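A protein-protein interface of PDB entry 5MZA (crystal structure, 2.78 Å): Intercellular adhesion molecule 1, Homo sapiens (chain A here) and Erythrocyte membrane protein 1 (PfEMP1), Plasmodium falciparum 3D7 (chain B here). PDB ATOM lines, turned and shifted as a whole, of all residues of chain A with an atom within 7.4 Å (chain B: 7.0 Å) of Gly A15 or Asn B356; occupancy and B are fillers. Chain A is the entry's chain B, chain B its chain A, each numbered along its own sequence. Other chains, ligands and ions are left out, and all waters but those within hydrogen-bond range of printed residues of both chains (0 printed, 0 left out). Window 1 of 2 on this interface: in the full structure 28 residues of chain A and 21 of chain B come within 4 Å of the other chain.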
ATOM      1  N   VAL A   9      37.963 -10.853  -8.626  1.00  0.00           N
ATOM      2  CA  VAL A   9      36.902 -11.618  -7.951  1.00  0.00           C
ATOM      3  C   VAL A   9      35.709 -11.865  -8.868  1.00  0.00           C
ATOM      4  O   VAL A   9      35.253 -10.947  -9.548  1.00  0.00           O
ATOM      5  CB  VAL A   9      36.432 -10.949  -6.616  1.00  0.00           C
ATOM      6  CG1 VAL A   9      35.320 -11.745  -5.937  1.00  0.00           C
ATOM      7  CG2 VAL A   9      37.586 -10.729  -5.647  1.00  0.00           C
ATOM      8  N   ILE A  10      35.184 -13.102  -8.847  1.00  0.00           N
ATOM      9  CA  ILE A  10      33.959 -13.500  -9.540  1.00  0.00           C
ATOM     10  C   ILE A  10      32.942 -13.880  -8.447  1.00  0.00           C
ATOM     11  O   ILE A  10      33.189 -14.798  -7.659  1.00  0.00           O
ATOM     12  CB  ILE A  10      34.146 -14.551 -10.695  1.00  0.00           C
ATOM     13  CG1 ILE A  10      32.818 -14.867 -11.429  1.00  0.00           C
ATOM     14  CG2 ILE A  10      34.851 -15.836 -10.245  1.00  0.00           C
ATOM     15  CD1 ILE A  10      32.439 -13.918 -12.550  1.00  0.00           C
ATOM     16  N   LEU A  11      31.855 -13.102  -8.337  1.00  0.00           N
ATOM     17  CA  LEU A  11      30.848 -13.314  -7.297  1.00  0.00           C
ATOM     18  C   LEU A  11      29.397 -13.148  -7.793  1.00  0.00           C
ATOM     19  O   LEU A  11      29.175 -12.437  -8.777  1.00  0.00           O
ATOM     20  CB  LEU A  11      31.136 -12.411  -6.067  1.00  0.00           C
ATOM     21  CG  LEU A  11      30.812 -10.908  -6.150  1.00  0.00           C
ATOM     22  CD1 LEU A  11      30.404 -10.381  -4.794  1.00  0.00           C
ATOM     23  CD2 LEU A  11      31.995 -10.107  -6.665  1.00  0.00           C
ATOM     24  N   PRO A  12      28.397 -13.796  -7.140  1.00  0.00           N
ATOM     25  CA  PRO A  12      27.001 -13.615  -7.585  1.00  0.00           C
ATOM     26  C   PRO A  12      26.485 -12.225  -7.203  1.00  0.00           C
ATOM     27  O   PRO A  12      26.974 -11.677  -6.211  1.00  0.00           O
ATOM     28  CB  PRO A  12      26.260 -14.738  -6.862  1.00  0.00           C
ATOM     29  CG  PRO A  12      27.058 -15.002  -5.644  1.00  0.00           C
ATOM     30  CD  PRO A  12      28.481 -14.683  -5.957  1.00  0.00           C
ATOM     31  N   ARG A  13      25.547 -11.625  -7.984  1.00  0.00           N
ATOM     32  CA  ARG A  13      25.116 -10.262  -7.651  1.00  0.00           C
ATOM     33  C   ARG A  13      24.214 -10.216  -6.409  1.00  0.00           C
ATOM     34  O   ARG A  13      23.382 -11.098  -6.183  1.00  0.00           O
ATOM     35  CB  ARG A  13      24.538  -9.472  -8.838  1.00  0.00           C
ATOM     36  CG  ARG A  13      23.116  -9.754  -9.227  1.00  0.00           C
ATOM     37  CD  ARG A  13      22.561  -8.606 -10.033  1.00  0.00           C
ATOM     38  NE  ARG A  13      21.289  -8.971 -10.651  1.00  0.00           N
ATOM     39  CZ  ARG A  13      20.767  -8.371 -11.713  1.00  0.00           C
ATOM     40  NH1 ARG A  13      21.403  -7.358 -12.292  1.00  0.00           N
ATOM     41  NH2 ARG A  13      19.609  -8.780 -12.209  1.00  0.00           N
ATOM     42  N   GLY A  14      24.465  -9.193  -5.601  1.00  0.00           N
ATOM     43  CA  GLY A  14      23.853  -8.982  -4.299  1.00  0.00           C
ATOM     44  C   GLY A  14      24.750  -9.605  -3.245  1.00  0.00           C
ATOM     45  O   GLY A  14      24.462  -9.530  -2.046  1.00  0.00           O
ATOM     46  N   GLY A  15      25.842 -10.217  -3.718  1.00  0.00           N
ATOM     47  CA  GLY A  15      26.828 -10.934  -2.921  1.00  0.00           C
ATOM     48  C   GLY A  15      27.824 -10.086  -2.170  1.00  0.00           C
ATOM     49  O   GLY A  15      27.853  -8.860  -2.310  1.00  0.00           O
ATOM     50  N   SER A  16      28.644 -10.757  -1.355  1.00  0.00           N
ATOM     51  CA  SER A  16      29.679 -10.131  -0.537  1.00  0.00           C
ATOM     52  C   SER A  16      31.086 -10.623  -0.889  1.00  0.00           C
ATOM     53  O   SER A  16      31.242 -11.686  -1.495  1.00  0.00           O
ATOM     54  CB  SER A  16      29.385 -10.324   0.947  1.00  0.00           C
ATOM     55  OG  SER A  16      28.161  -9.704   1.300  1.00  0.00           O
ATOM     56  N   VAL A  17      32.104  -9.824  -0.529  1.00  0.00           N
ATOM     57  CA  VAL A  17      33.522 -10.119  -0.763  1.00  0.00           C
ATOM     58  C   VAL A  17      34.386  -9.546   0.372  1.00  0.00           C
ATOM     59  O   VAL A  17      34.059  -8.503   0.942  1.00  0.00           O
ATOM     60  CB  VAL A  17      33.998  -9.699  -2.191  1.00  0.00           C
ATOM     61  CG1 VAL A  17      33.903  -8.190  -2.412  1.00  0.00           C
ATOM     62  CG2 VAL A  17      35.401 -10.216  -2.504  1.00  0.00           C
ATOM     63  N   LEU A  18      35.467 -10.254   0.711  1.00  0.00           N
ATOM     64  CA  LEU A  18      36.418  -9.852   1.736  1.00  0.00           C
ATOM     65  C   LEU A  18      37.654  -9.305   1.023  1.00  0.00           C
ATOM     66  O   LEU A  18      38.341 -10.054   0.321  1.00  0.00           O
ATOM     67  CB  LEU A  18      36.767 -11.060   2.628  1.00  0.00           C
ATOM     68  CG  LEU A  18      37.311 -10.754   4.018  1.00  0.00           C
ATOM     69  CD1 LEU A  18      36.216 -10.227   4.943  1.00  0.00           C
ATOM     70  CD2 LEU A  18      37.964 -11.979   4.628  1.00  0.00           C
ATOM     71  N   LEU A  37      29.981   0.770  -2.105  1.00  0.00           N
ATOM     72  CA  LEU A  37      29.402  -0.489  -1.628  1.00  0.00           C
ATOM     73  C   LEU A  37      29.378  -0.511  -0.095  1.00  0.00           C
ATOM     74  O   LEU A  37      30.356  -0.061   0.511  1.00  0.00           O
ATOM     75  CB  LEU A  37      30.228  -1.702  -2.116  1.00  0.00           C
ATOM     76  CG  LEU A  37      30.269  -2.009  -3.612  1.00  0.00           C
ATOM     77  CD1 LEU A  37      31.407  -2.950  -3.929  1.00  0.00           C
ATOM     78  CD2 LEU A  37      28.961  -2.600  -4.096  1.00  0.00           C
ATOM     79  N   LEU A  54      32.720  -6.189   1.831  1.00  0.00           N
ATOM     80  CA  LEU A  54      31.891  -5.440   0.893  1.00  0.00           C
ATOM     81  C   LEU A  54      30.641  -6.239   0.590  1.00  0.00           C
ATOM     82  O   LEU A  54      30.743  -7.360   0.098  1.00  0.00           O
ATOM     83  CB  LEU A  54      32.682  -5.130  -0.392  1.00  0.00           C
ATOM     84  CG  LEU A  54      34.014  -4.397  -0.207  1.00  0.00           C
ATOM     85  CD1 LEU A  54      34.834  -4.445  -1.466  1.00  0.00           C
ATOM     86  CD2 LEU A  54      33.802  -2.964   0.240  1.00  0.00           C
ATOM     87  N   SER A  55      29.466  -5.690   0.931  1.00  0.00           N
ATOM     88  CA  SER A  55      28.189  -6.371   0.714  1.00  0.00           C
ATOM     89  C   SER A  55      27.360  -5.712  -0.379  1.00  0.00           C
ATOM     90  O   SER A  55      27.731  -4.643  -0.864  1.00  0.00           O
ATOM     91  CB  SER A  55      27.401  -6.470   2.018  1.00  0.00           C
ATOM     92  OG  SER A  55      27.134  -5.195   2.577  1.00  0.00           O
ATOM     93  N   ASN A  56      26.258  -6.377  -0.792  1.00  0.00           N
ATOM     94  CA  ASN A  56      25.292  -5.927  -1.802  1.00  0.00           C
ATOM     95  C   ASN A  56      25.956  -5.490  -3.130  1.00  0.00           C
ATOM     96  O   ASN A  56      25.613  -4.438  -3.682  1.00  0.00           O
ATOM     97  CB  ASN A  56      24.378  -4.829  -1.211  1.00  0.00           C
ATOM     98  CG  ASN A  56      23.061  -4.629  -1.923  1.00  0.00           C
ATOM     99  OD1 ASN A  56      22.394  -5.579  -2.359  1.00  0.00           O
ATOM    100  ND2 ASN A  56      22.628  -3.381  -2.003  1.00  0.00           N
ATOM    101  N   VAL A  57      26.916  -6.302  -3.633  1.00  0.00           N
ATOM    102  CA  VAL A  57      27.620  -6.019  -4.894  1.00  0.00           C
ATOM    103  C   VAL A  57      26.649  -6.322  -6.040  1.00  0.00           C
ATOM    104  O   VAL A  57      26.495  -7.478  -6.437  1.00  0.00           O
ATOM    105  CB  VAL A  57      28.985  -6.759  -5.037  1.00  0.00           C
ATOM    106  CG1 VAL A  57      29.742  -6.285  -6.276  1.00  0.00           C
ATOM    107  CG2 VAL A  57      29.849  -6.589  -3.790  1.00  0.00           C
ATOM    108  N   GLN A  58      25.951  -5.285  -6.524  1.00  0.00           N
ATOM    109  CA  GLN A  58      24.944  -5.417  -7.579  1.00  0.00           C
ATOM    110  C   GLN A  58      25.516  -5.413  -8.997  1.00  0.00           C
ATOM    111  O   GLN A  58      24.989  -6.115  -9.865  1.00  0.00           O
ATOM    112  CB  GLN A  58      23.850  -4.348  -7.429  1.00  0.00           C
ATOM    113  CG  GLN A  58      22.967  -4.529  -6.190  1.00  0.00           C
ATOM    114  CD  GLN A  58      22.106  -5.775  -6.194  1.00  0.00           C
ATOM    115  OE1 GLN A  58      21.697  -6.298  -7.239  1.00  0.00           O
ATOM    116  NE2 GLN A  58      21.778  -6.255  -5.008  1.00  0.00           N
ATOM    117  N   LEU A  80      36.009  -6.529  -9.365  1.00  0.00           N
ATOM    118  CA  LEU A  80      34.828  -7.322  -9.037  1.00  0.00           C
ATOM    119  C   LEU A  80      34.008  -7.543 -10.303  1.00  0.00           C
ATOM    120  O   LEU A  80      33.589  -6.580 -10.956  1.00  0.00           O
ATOM    121  CB  LEU A  80      33.952  -6.666  -7.940  1.00  0.00           C
ATOM    122  CG  LEU A  80      34.592  -6.251  -6.608  1.00  0.00           C
ATOM    123  CD1 LEU A  80      33.554  -5.645  -5.692  1.00  0.00           C
ATOM    124  CD2 LEU A  80      35.242  -7.423  -5.898  1.00  0.00           C
ATOM    125  N   VAL A  82      30.672  -9.305 -11.391  1.00  0.00           N
ATOM    126  CA  VAL A  82      29.400  -9.814 -10.905  1.00  0.00           C
ATOM    127  C   VAL A  82      28.740 -10.731 -11.950  1.00  0.00           C
ATOM    128  O   VAL A  82      28.961 -10.554 -13.151  1.00  0.00           O
ATOM    129  CB  VAL A  82      28.518  -8.625 -10.432  1.00  0.00           C
ATOM    130  CG1 VAL A  82      27.197  -8.503 -11.198  1.00  0.00           C
ATOM    131  CG2 VAL A  82      28.290  -8.681  -8.930  1.00  0.00           C
ATOM    132  N   TYR A  83      27.975 -11.734 -11.486  1.00  0.00           N
ATOM    133  CA  TYR A  83      27.254 -12.647 -12.373  1.00  0.00           C
ATOM    134  C   TYR A  83      25.821 -12.859 -11.909  1.00  0.00           C
ATOM    135  O   TYR A  83      25.529 -12.778 -10.711  1.00  0.00           O
ATOM    136  CB  TYR A  83      28.001 -13.975 -12.617  1.00  0.00           C
ATOM    137  CG  TYR A  83      27.918 -14.979 -11.492  1.00  0.00           C
ATOM    138  CD1 TYR A  83      26.802 -15.800 -11.345  1.00  0.00           C
ATOM    139  CD2 TYR A  83      28.984 -15.167 -10.620  1.00  0.00           C
ATOM    140  CE1 TYR A  83      26.720 -16.730 -10.313  1.00  0.00           C
ATOM    141  CE2 TYR A  83      28.918 -16.101  -9.589  1.00  0.00           C
ATOM    142  CZ  TYR A  83      27.784 -16.880  -9.441  1.00  0.00           C
ATOM    143  OH  TYR A  83      27.710 -17.805  -8.437  1.00  0.00           O
ATOM    144  N   ARG B 351      31.500 -17.542   6.173  1.00  0.00           N
ATOM    145  CA  ARG B 351      30.217 -16.847   6.220  1.00  0.00           C
ATOM    146  C   ARG B 351      29.913 -16.201   4.873  1.00  0.00           C
ATOM    147  O   ARG B 351      28.780 -16.311   4.410  1.00  0.00           O
ATOM    148  CB  ARG B 351      30.197 -15.815   7.358  1.00  0.00           C
ATOM    149  CG  ARG B 351      28.874 -15.051   7.508  1.00  0.00           C
ATOM    150  CD  ARG B 351      28.822 -14.159   8.741  1.00  0.00           C
ATOM    151  NE  ARG B 351      30.064 -13.405   8.930  1.00  0.00           N
ATOM    152  CZ  ARG B 351      30.365 -12.273   8.303  1.00  0.00           C
ATOM    153  NH1 ARG B 351      29.503 -11.727   7.449  1.00  0.00           N
ATOM    154  NH2 ARG B 351      31.527 -11.673   8.527  1.00  0.00           N
ATOM    155  N   ILE B 352      30.921 -15.562   4.233  1.00  0.00           N
ATOM    156  CA  ILE B 352      30.773 -14.925   2.915  1.00  0.00           C
ATOM    157  C   ILE B 352      30.427 -15.987   1.855  1.00  0.00           C
ATOM    158  O   ILE B 352      29.514 -15.762   1.057  1.00  0.00           O
ATOM    159  CB  ILE B 352      31.989 -14.017   2.550  1.00  0.00           C
ATOM    160  CG1 ILE B 352      31.945 -12.709   3.377  1.00  0.00           C
ATOM    161  CG2 ILE B 352      32.053 -13.702   1.044  1.00  0.00           C
ATOM    162  CD1 ILE B 352      33.256 -12.032   3.572  1.00  0.00           C
ATOM    163  N   THR B 353      31.099 -17.166   1.905  1.00  0.00           N
ATOM    164  CA  THR B 353      30.833 -18.295   1.005  1.00  0.00           C
ATOM    165  C   THR B 353      29.347 -18.670   1.090  1.00  0.00           C
ATOM    166  O   THR B 353      28.703 -18.784   0.054  1.00  0.00           O
ATOM    167  CB  THR B 353      31.773 -19.489   1.301  1.00  0.00           C
ATOM    168  OG1 THR B 353      33.125 -19.044   1.278  1.00  0.00           O
ATOM    169  CG2 THR B 353      31.624 -20.621   0.291  1.00  0.00           C
ATOM    170  N   ALA B 354      28.798 -18.767   2.320  1.00  0.00           N
ATOM    171  CA  ALA B 354      27.394 -19.082   2.600  1.00  0.00           C
ATOM    172  C   ALA B 354      26.418 -18.024   2.089  1.00  0.00           C
ATOM    173  O   ALA B 354      25.384 -18.381   1.522  1.00  0.00           O
ATOM    174  CB  ALA B 354      27.205 -19.289   4.083  1.00  0.00           C
ATOM    175  N   ILE B 355      26.754 -16.729   2.270  1.00  0.00           N
ATOM    176  CA  ILE B 355      25.976 -15.584   1.792  1.00  0.00           C
ATOM    177  C   ILE B 355      25.895 -15.649   0.253  1.00  0.00           C
ATOM    178  O   ILE B 355      24.845 -15.363  -0.327  1.00  0.00           O
ATOM    179  CB  ILE B 355      26.632 -14.256   2.302  1.00  0.00           C
ATOM    180  CG1 ILE B 355      26.382 -14.061   3.817  1.00  0.00           C
ATOM    181  CG2 ILE B 355      26.185 -13.014   1.494  1.00  0.00           C
ATOM    182  CD1 ILE B 355      27.404 -13.163   4.553  1.00  0.00           C
ATOM    183  N   ASN B 356      27.004 -16.057  -0.389  1.00  0.00           N
ATOM    184  CA  ASN B 356      27.112 -16.138  -1.841  1.00  0.00           C
ATOM    185  C   ASN B 356      26.473 -17.400  -2.457  1.00  0.00           C
ATOM    186  O   ASN B 356      26.226 -17.419  -3.661  1.00  0.00           O
ATOM    187  CB  ASN B 356      28.569 -15.956  -2.277  1.00  0.00           C
ATOM    188  CG  ASN B 356      29.083 -14.537  -2.077  1.00  0.00           C
ATOM    189  OD1 ASN B 356      28.339 -13.601  -1.760  1.00  0.00           O
ATOM    190  ND2 ASN B 356      30.373 -14.335  -2.257  1.00  0.00           N
ATOM    191  N   GLY B 357      26.145 -18.392  -1.631  1.00  0.00           N
ATOM    192  CA  GLY B 357      25.486 -19.613  -2.087  1.00  0.00           C
ATOM    193  C   GLY B 357      26.306 -20.882  -1.998  1.00  0.00           C
ATOM    194  O   GLY B 357      25.963 -21.887  -2.622  1.00  0.00           O
ATOM    195  N   GLY B 358      27.371 -20.828  -1.211  1.00  0.00           N
ATOM    196  CA  GLY B 358      28.293 -21.932  -0.985  1.00  0.00           C
ATOM    197  C   GLY B 358      29.176 -22.249  -2.172  1.00  0.00           C
ATOM    198  O   GLY B 358      29.315 -21.414  -3.075  1.00  0.00           O
ATOM    199  N   PRO B 359      29.774 -23.467  -2.209  1.00  0.00           N
ATOM    200  CA  PRO B 359      30.599 -23.852  -3.370  1.00  0.00           C
ATOM    201  C   PRO B 359      29.742 -23.938  -4.633  1.00  0.00           C
ATOM    202  O   PRO B 359      28.516 -24.091  -4.548  1.00  0.00           O
ATOM    203  CB  PRO B 359      31.154 -25.229  -2.976  1.00  0.00           C
ATOM    204  CG  PRO B 359      30.948 -25.331  -1.500  1.00  0.00           C
ATOM    205  CD  PRO B 359      29.697 -24.565  -1.228  1.00  0.00           C
ATOM    206  N   GLY B 360      30.379 -23.788  -5.789  1.00  0.00           N
ATOM    207  CA  GLY B 360      29.679 -23.772  -7.070  1.00  0.00           C
ATOM    208  C   GLY B 360      29.204 -22.374  -7.422  1.00  0.00           C
ATOM    209  O   GLY B 360      29.090 -22.033  -8.599  1.00  0.00           O
ATOM    210  N   TYR B 361      28.937 -21.555  -6.387  1.00  0.00           N
ATOM    211  CA  TYR B 361      28.525 -20.157  -6.484  1.00  0.00           C
ATOM    212  C   TYR B 361      29.684 -19.204  -6.160  1.00  0.00           C
ATOM    213  O   TYR B 361      29.732 -18.100  -6.707  1.00  0.00           O
ATOM    214  CB  TYR B 361      27.331 -19.867  -5.556  1.00  0.00           C
ATOM    215  CG  TYR B 361      25.985 -20.253  -6.133  1.00  0.00           C
ATOM    216  CD1 TYR B 361      25.282 -19.380  -6.956  1.00  0.00           C
ATOM    217  CD2 TYR B 361      25.397 -21.476  -5.825  1.00  0.00           C
ATOM    218  CE1 TYR B 361      24.045 -19.730  -7.492  1.00  0.00           C
ATOM    219  CE2 TYR B 361      24.154 -21.834  -6.346  1.00  0.00           C
ATOM    220  CZ  TYR B 361      23.479 -20.957  -7.180  1.00  0.00           C
ATOM    221  OH  TYR B 361      22.257 -21.312  -7.706  1.00  0.00           O
ATOM    222  N   TYR B 362      30.618 -19.622  -5.278  1.00  0.00           N
ATOM    223  CA  TYR B 362      31.740 -18.768  -4.874  1.00  0.00           C
ATOM    224  C   TYR B 362      32.989 -19.525  -4.431  1.00  0.00           C
ATOM    225  O   TYR B 362      32.923 -20.386  -3.547  1.00  0.00           O
ATOM    226  CB  TYR B 362      31.288 -17.777  -3.780  1.00  0.00           C
ATOM    227  CG  TYR B 362      32.314 -16.742  -3.374  1.00  0.00           C
ATOM    228  CD1 TYR B 362      32.760 -15.780  -4.278  1.00  0.00           C
ATOM    229  CD2 TYR B 362      32.776 -16.668  -2.064  1.00  0.00           C
ATOM    230  CE1 TYR B 362      33.689 -14.808  -3.902  1.00  0.00           C
ATOM    231  CE2 TYR B 362      33.693 -15.694  -1.673  1.00  0.00           C
ATOM    232  CZ  TYR B 362      34.149 -14.767  -2.596  1.00  0.00           C
ATOM    233  OH  TYR B 362      35.057 -13.810  -2.209  1.00  0.00           O
ATOM    234  N   ASN B 363      34.137 -19.162  -5.037  1.00  0.00           N
ATOM    235  CA  ASN B 363      35.452 -19.719  -4.720  1.00  0.00           C
ATOM    236  C   ASN B 363      36.245 -18.669  -3.964  1.00  0.00           C
ATOM    237  O   ASN B 363      36.695 -17.684  -4.548  1.00  0.00           O
ATOM    238  CB  ASN B 363      36.200 -20.177  -5.981  1.00  0.00           C
ATOM    239  CG  ASN B 363      35.767 -21.511  -6.529  1.00  0.00           C
ATOM    240  OD1 ASN B 363      35.435 -22.453  -5.791  1.00  0.00           O
ATOM    241  ND2 ASN B 363      35.808 -21.630  -7.849  1.00  0.00           N
ATOM    242  N   LYS B 387      22.149 -18.221   7.055  1.00  0.00           N
ATOM    243  CA  LYS B 387      21.359 -18.249   5.821  1.00  0.00           C
ATOM    244  C   LYS B 387      22.199 -18.579   4.580  1.00  0.00           C
ATOM    245  O   LYS B 387      23.098 -17.816   4.217  1.00  0.00           O
ATOM    246  CB  LYS B 387      20.563 -16.938   5.628  1.00  0.00           C
ATOM    247  CG  LYS B 387      19.634 -16.561   6.787  1.00  0.00           C
ATOM    248  CD  LYS B 387      18.313 -17.324   6.783  1.00  0.00           C
ATOM    249  CE  LYS B 387      17.466 -16.956   7.975  1.00  0.00           C
ATOM    250  NZ  LYS B 387      16.121 -17.588   7.914  1.00  0.00           N
ATOM    251  N   LYS B 388      21.886 -19.718   3.932  1.00  0.00           N
ATOM    252  CA  LYS B 388      22.537 -20.215   2.715  1.00  0.00           C
ATOM    253  C   LYS B 388      21.892 -19.583   1.462  1.00  0.00           C
ATOM    254  O   LYS B 388      21.182 -18.573   1.555  1.00  0.00           O
ATOM    255  CB  LYS B 388      22.408 -21.752   2.651  1.00  0.00           C
ATOM    256  CG  LYS B 388      23.461 -22.449   1.783  1.00  0.00           C
ATOM    257  CD  LYS B 388      22.885 -23.683   1.119  1.00  0.00           C
ATOM    258  CE  LYS B 388      23.876 -24.376   0.224  1.00  0.00           C
ATOM    259  NZ  LYS B 388      23.316 -25.639  -0.329  1.00  0.00           N
ATOM    260  N   GLY B 389      22.161 -20.199   0.307  1.00  0.00           N
ATOM    261  CA  GLY B 389      21.630 -19.817  -0.990  1.00  0.00           C
ATOM    262  C   GLY B 389      22.187 -18.521  -1.533  1.00  0.00           C
ATOM    263  O   GLY B 389      22.529 -17.614  -0.763  1.00  0.00           O
ATOM    264  N   PRO B 390      22.276 -18.401  -2.877  1.00  0.00           N
ATOM    265  CA  PRO B 390      22.759 -17.147  -3.467  1.00  0.00           C
ATOM    266  C   PRO B 390      21.829 -15.981  -3.116  1.00  0.00           C
ATOM    267  O   PRO B 390      20.648 -16.229  -2.835  1.00  0.00           O
ATOM    268  CB  PRO B 390      22.727 -17.437  -4.974  1.00  0.00           C
ATOM    269  CG  PRO B 390      21.709 -18.511  -5.131  1.00  0.00           C
ATOM    270  CD  PRO B 390      21.900 -19.371  -3.925  1.00  0.00           C
ATOM    271  N   PRO B 391      22.310 -14.714  -3.138  1.00  0.00           N
ATOM    272  CA  PRO B 391      21.420 -13.580  -2.829  1.00  0.00           C
ATOM    273  C   PRO B 391      20.197 -13.520  -3.755  1.00  0.00           C
ATOM    274  O   PRO B 391      20.254 -14.096  -4.847  1.00  0.00           O
ATOM    275  CB  PRO B 391      22.330 -12.365  -3.023  1.00  0.00           C
ATOM    276  CG  PRO B 391      23.697 -12.890  -2.831  1.00  0.00           C
ATOM    277  CD  PRO B 391      23.677 -14.242  -3.440  1.00  0.00           C
ATOM    278  N   ASP B 393      19.199 -11.326  -5.785  1.00  0.00           N
ATOM    279  CA  ASP B 393      19.513 -10.664  -7.047  1.00  0.00           C
ATOM    280  C   ASP B 393      20.257 -11.551  -8.055  1.00  0.00           C
ATOM    281  O   ASP B 393      20.315 -11.191  -9.229  1.00  0.00           O
ATOM    282  CB  ASP B 393      20.254  -9.342  -6.808  1.00  0.00           C
ATOM    283  CG  ASP B 393      19.373  -8.283  -6.176  1.00  0.00           C
ATOM    284  OD1 ASP B 393      18.464  -7.771  -6.871  1.00  0.00           O
ATOM    285  OD2 ASP B 393      19.576  -7.981  -4.982  1.00  0.00           O
ATOM    286  N   THR B 394      20.776 -12.716  -7.626  1.00  0.00           N
ATOM    287  CA  THR B 394      21.496 -13.660  -8.496  1.00  0.00           C
ATOM    288  C   THR B 394      20.557 -14.321  -9.527  1.00  0.00           C
ATOM    289  O   THR B 394      20.837 -14.273 -10.728  1.00  0.00           O
ATOM    290  CB  THR B 394      22.279 -14.662  -7.648  1.00  0.00           C
ATOM    291  OG1 THR B 394      23.153 -13.927  -6.796  1.00  0.00           O
ATOM    292  CG2 THR B 394      23.078 -15.651  -8.490  1.00  0.00           C
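OD1 of Asn B356 lies within hydrogen-bond range of N of Ser A16, 2.9 Å away. O of Asp B393 lies within hydrogen-bond range of NE of Arg A13 (2.8 Å). The side-chain hydroxyl (OG1) of Thr B394 lies within hydrogen-bond range of the backbone carbonyl oxygen (O) of Arg A13, at 2.9 Å. The side-chain carboxylate of Asp B393 lies within hydrogen-bond range of the side-chain amide nitrogen of Gln A58, at 2.8 Å. O of Tyr B361 is in hydrogen-bond range of OH of Tyr A83 (2.7 Å).
Printed residues of chain B that touch a printed residue of chain A: Ile B352, Ile B355, Asn B356, Tyr B361, Tyr B362, Pro B391, Asp B393 and Thr B394. Of the 19 printed residues of chain A, 10 touch a printed residue of chain B. Hydrophobic or aromatic side chains of chain A within 4 Å of the printed part of chain B: Pro A12, Val A17, Leu A18 and Tyr A83. Among the printed residues, no Asp or Glu carboxylate lies within 4 Å of a Lys or Arg side-chain nitrogen of the other chain.
N of Val A57 lies within hydrogen-bond range of O of Gly A15 (3.0 Å). The backbone NH (N) of Gly A14 lies within hydrogen-bond range of the backbone carbonyl oxygen (O) of Val A57 (2.8 Å). The side-chain amide oxygen (OD1) of Asn A56 lies within hydrogen-bond range of the side-chain amide nitrogen (NE2) of Gln A58 (2.8 Å). N of Arg A13 lies within hydrogen-bond range of O of Tyr A83, 3.0 Å away. N of Leu A54 sits at hydrogen-bond distance from O of Val A17, 2.8 Å away. The backbone carbonyl oxygen (O) of Leu A11 lies within hydrogen-bond range of the backbone NH (N) of Tyr A83.
Gly A14 touches just one residue of chain B: Pro B391. Of the printed residues of chain A, Ile B355 touches Ser A16. Of the printed residues of chain A, Pro B391 touches Arg A13, Gly A14 and Gly A15. Of the printed residues of chain B, Pro A12 touches Asn B356, Tyr B361 and Thr B394. The nearest residue of chain A that does not touch Asn B356 is Leu A11 (4.3 Å).
Among the printed residues, merely in contact across the chains: Ile A10 with Tyr B362 (3.5 Å), Pro A12 with Asn B356 (3.2 Å), Pro A12 with Tyr B361 (3.7 Å), Pro A12 with Thr B394 (3.2 Å), Arg A13 with Pro B391 (3.6 Å), Gly A14 with Pro B391 (3.5 Å), Gly A15 with Asn B356 (3.3 Å), Gly A15 with Pro B391 (3.5 Å), Ser A16 with Ile B352 (3.3 Å), Ser A16 with Ile B355 (3.9 Å), Val A17 with Tyr B362 (3.6 Å) and Leu A18 with Ile B352 (3.7 Å).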
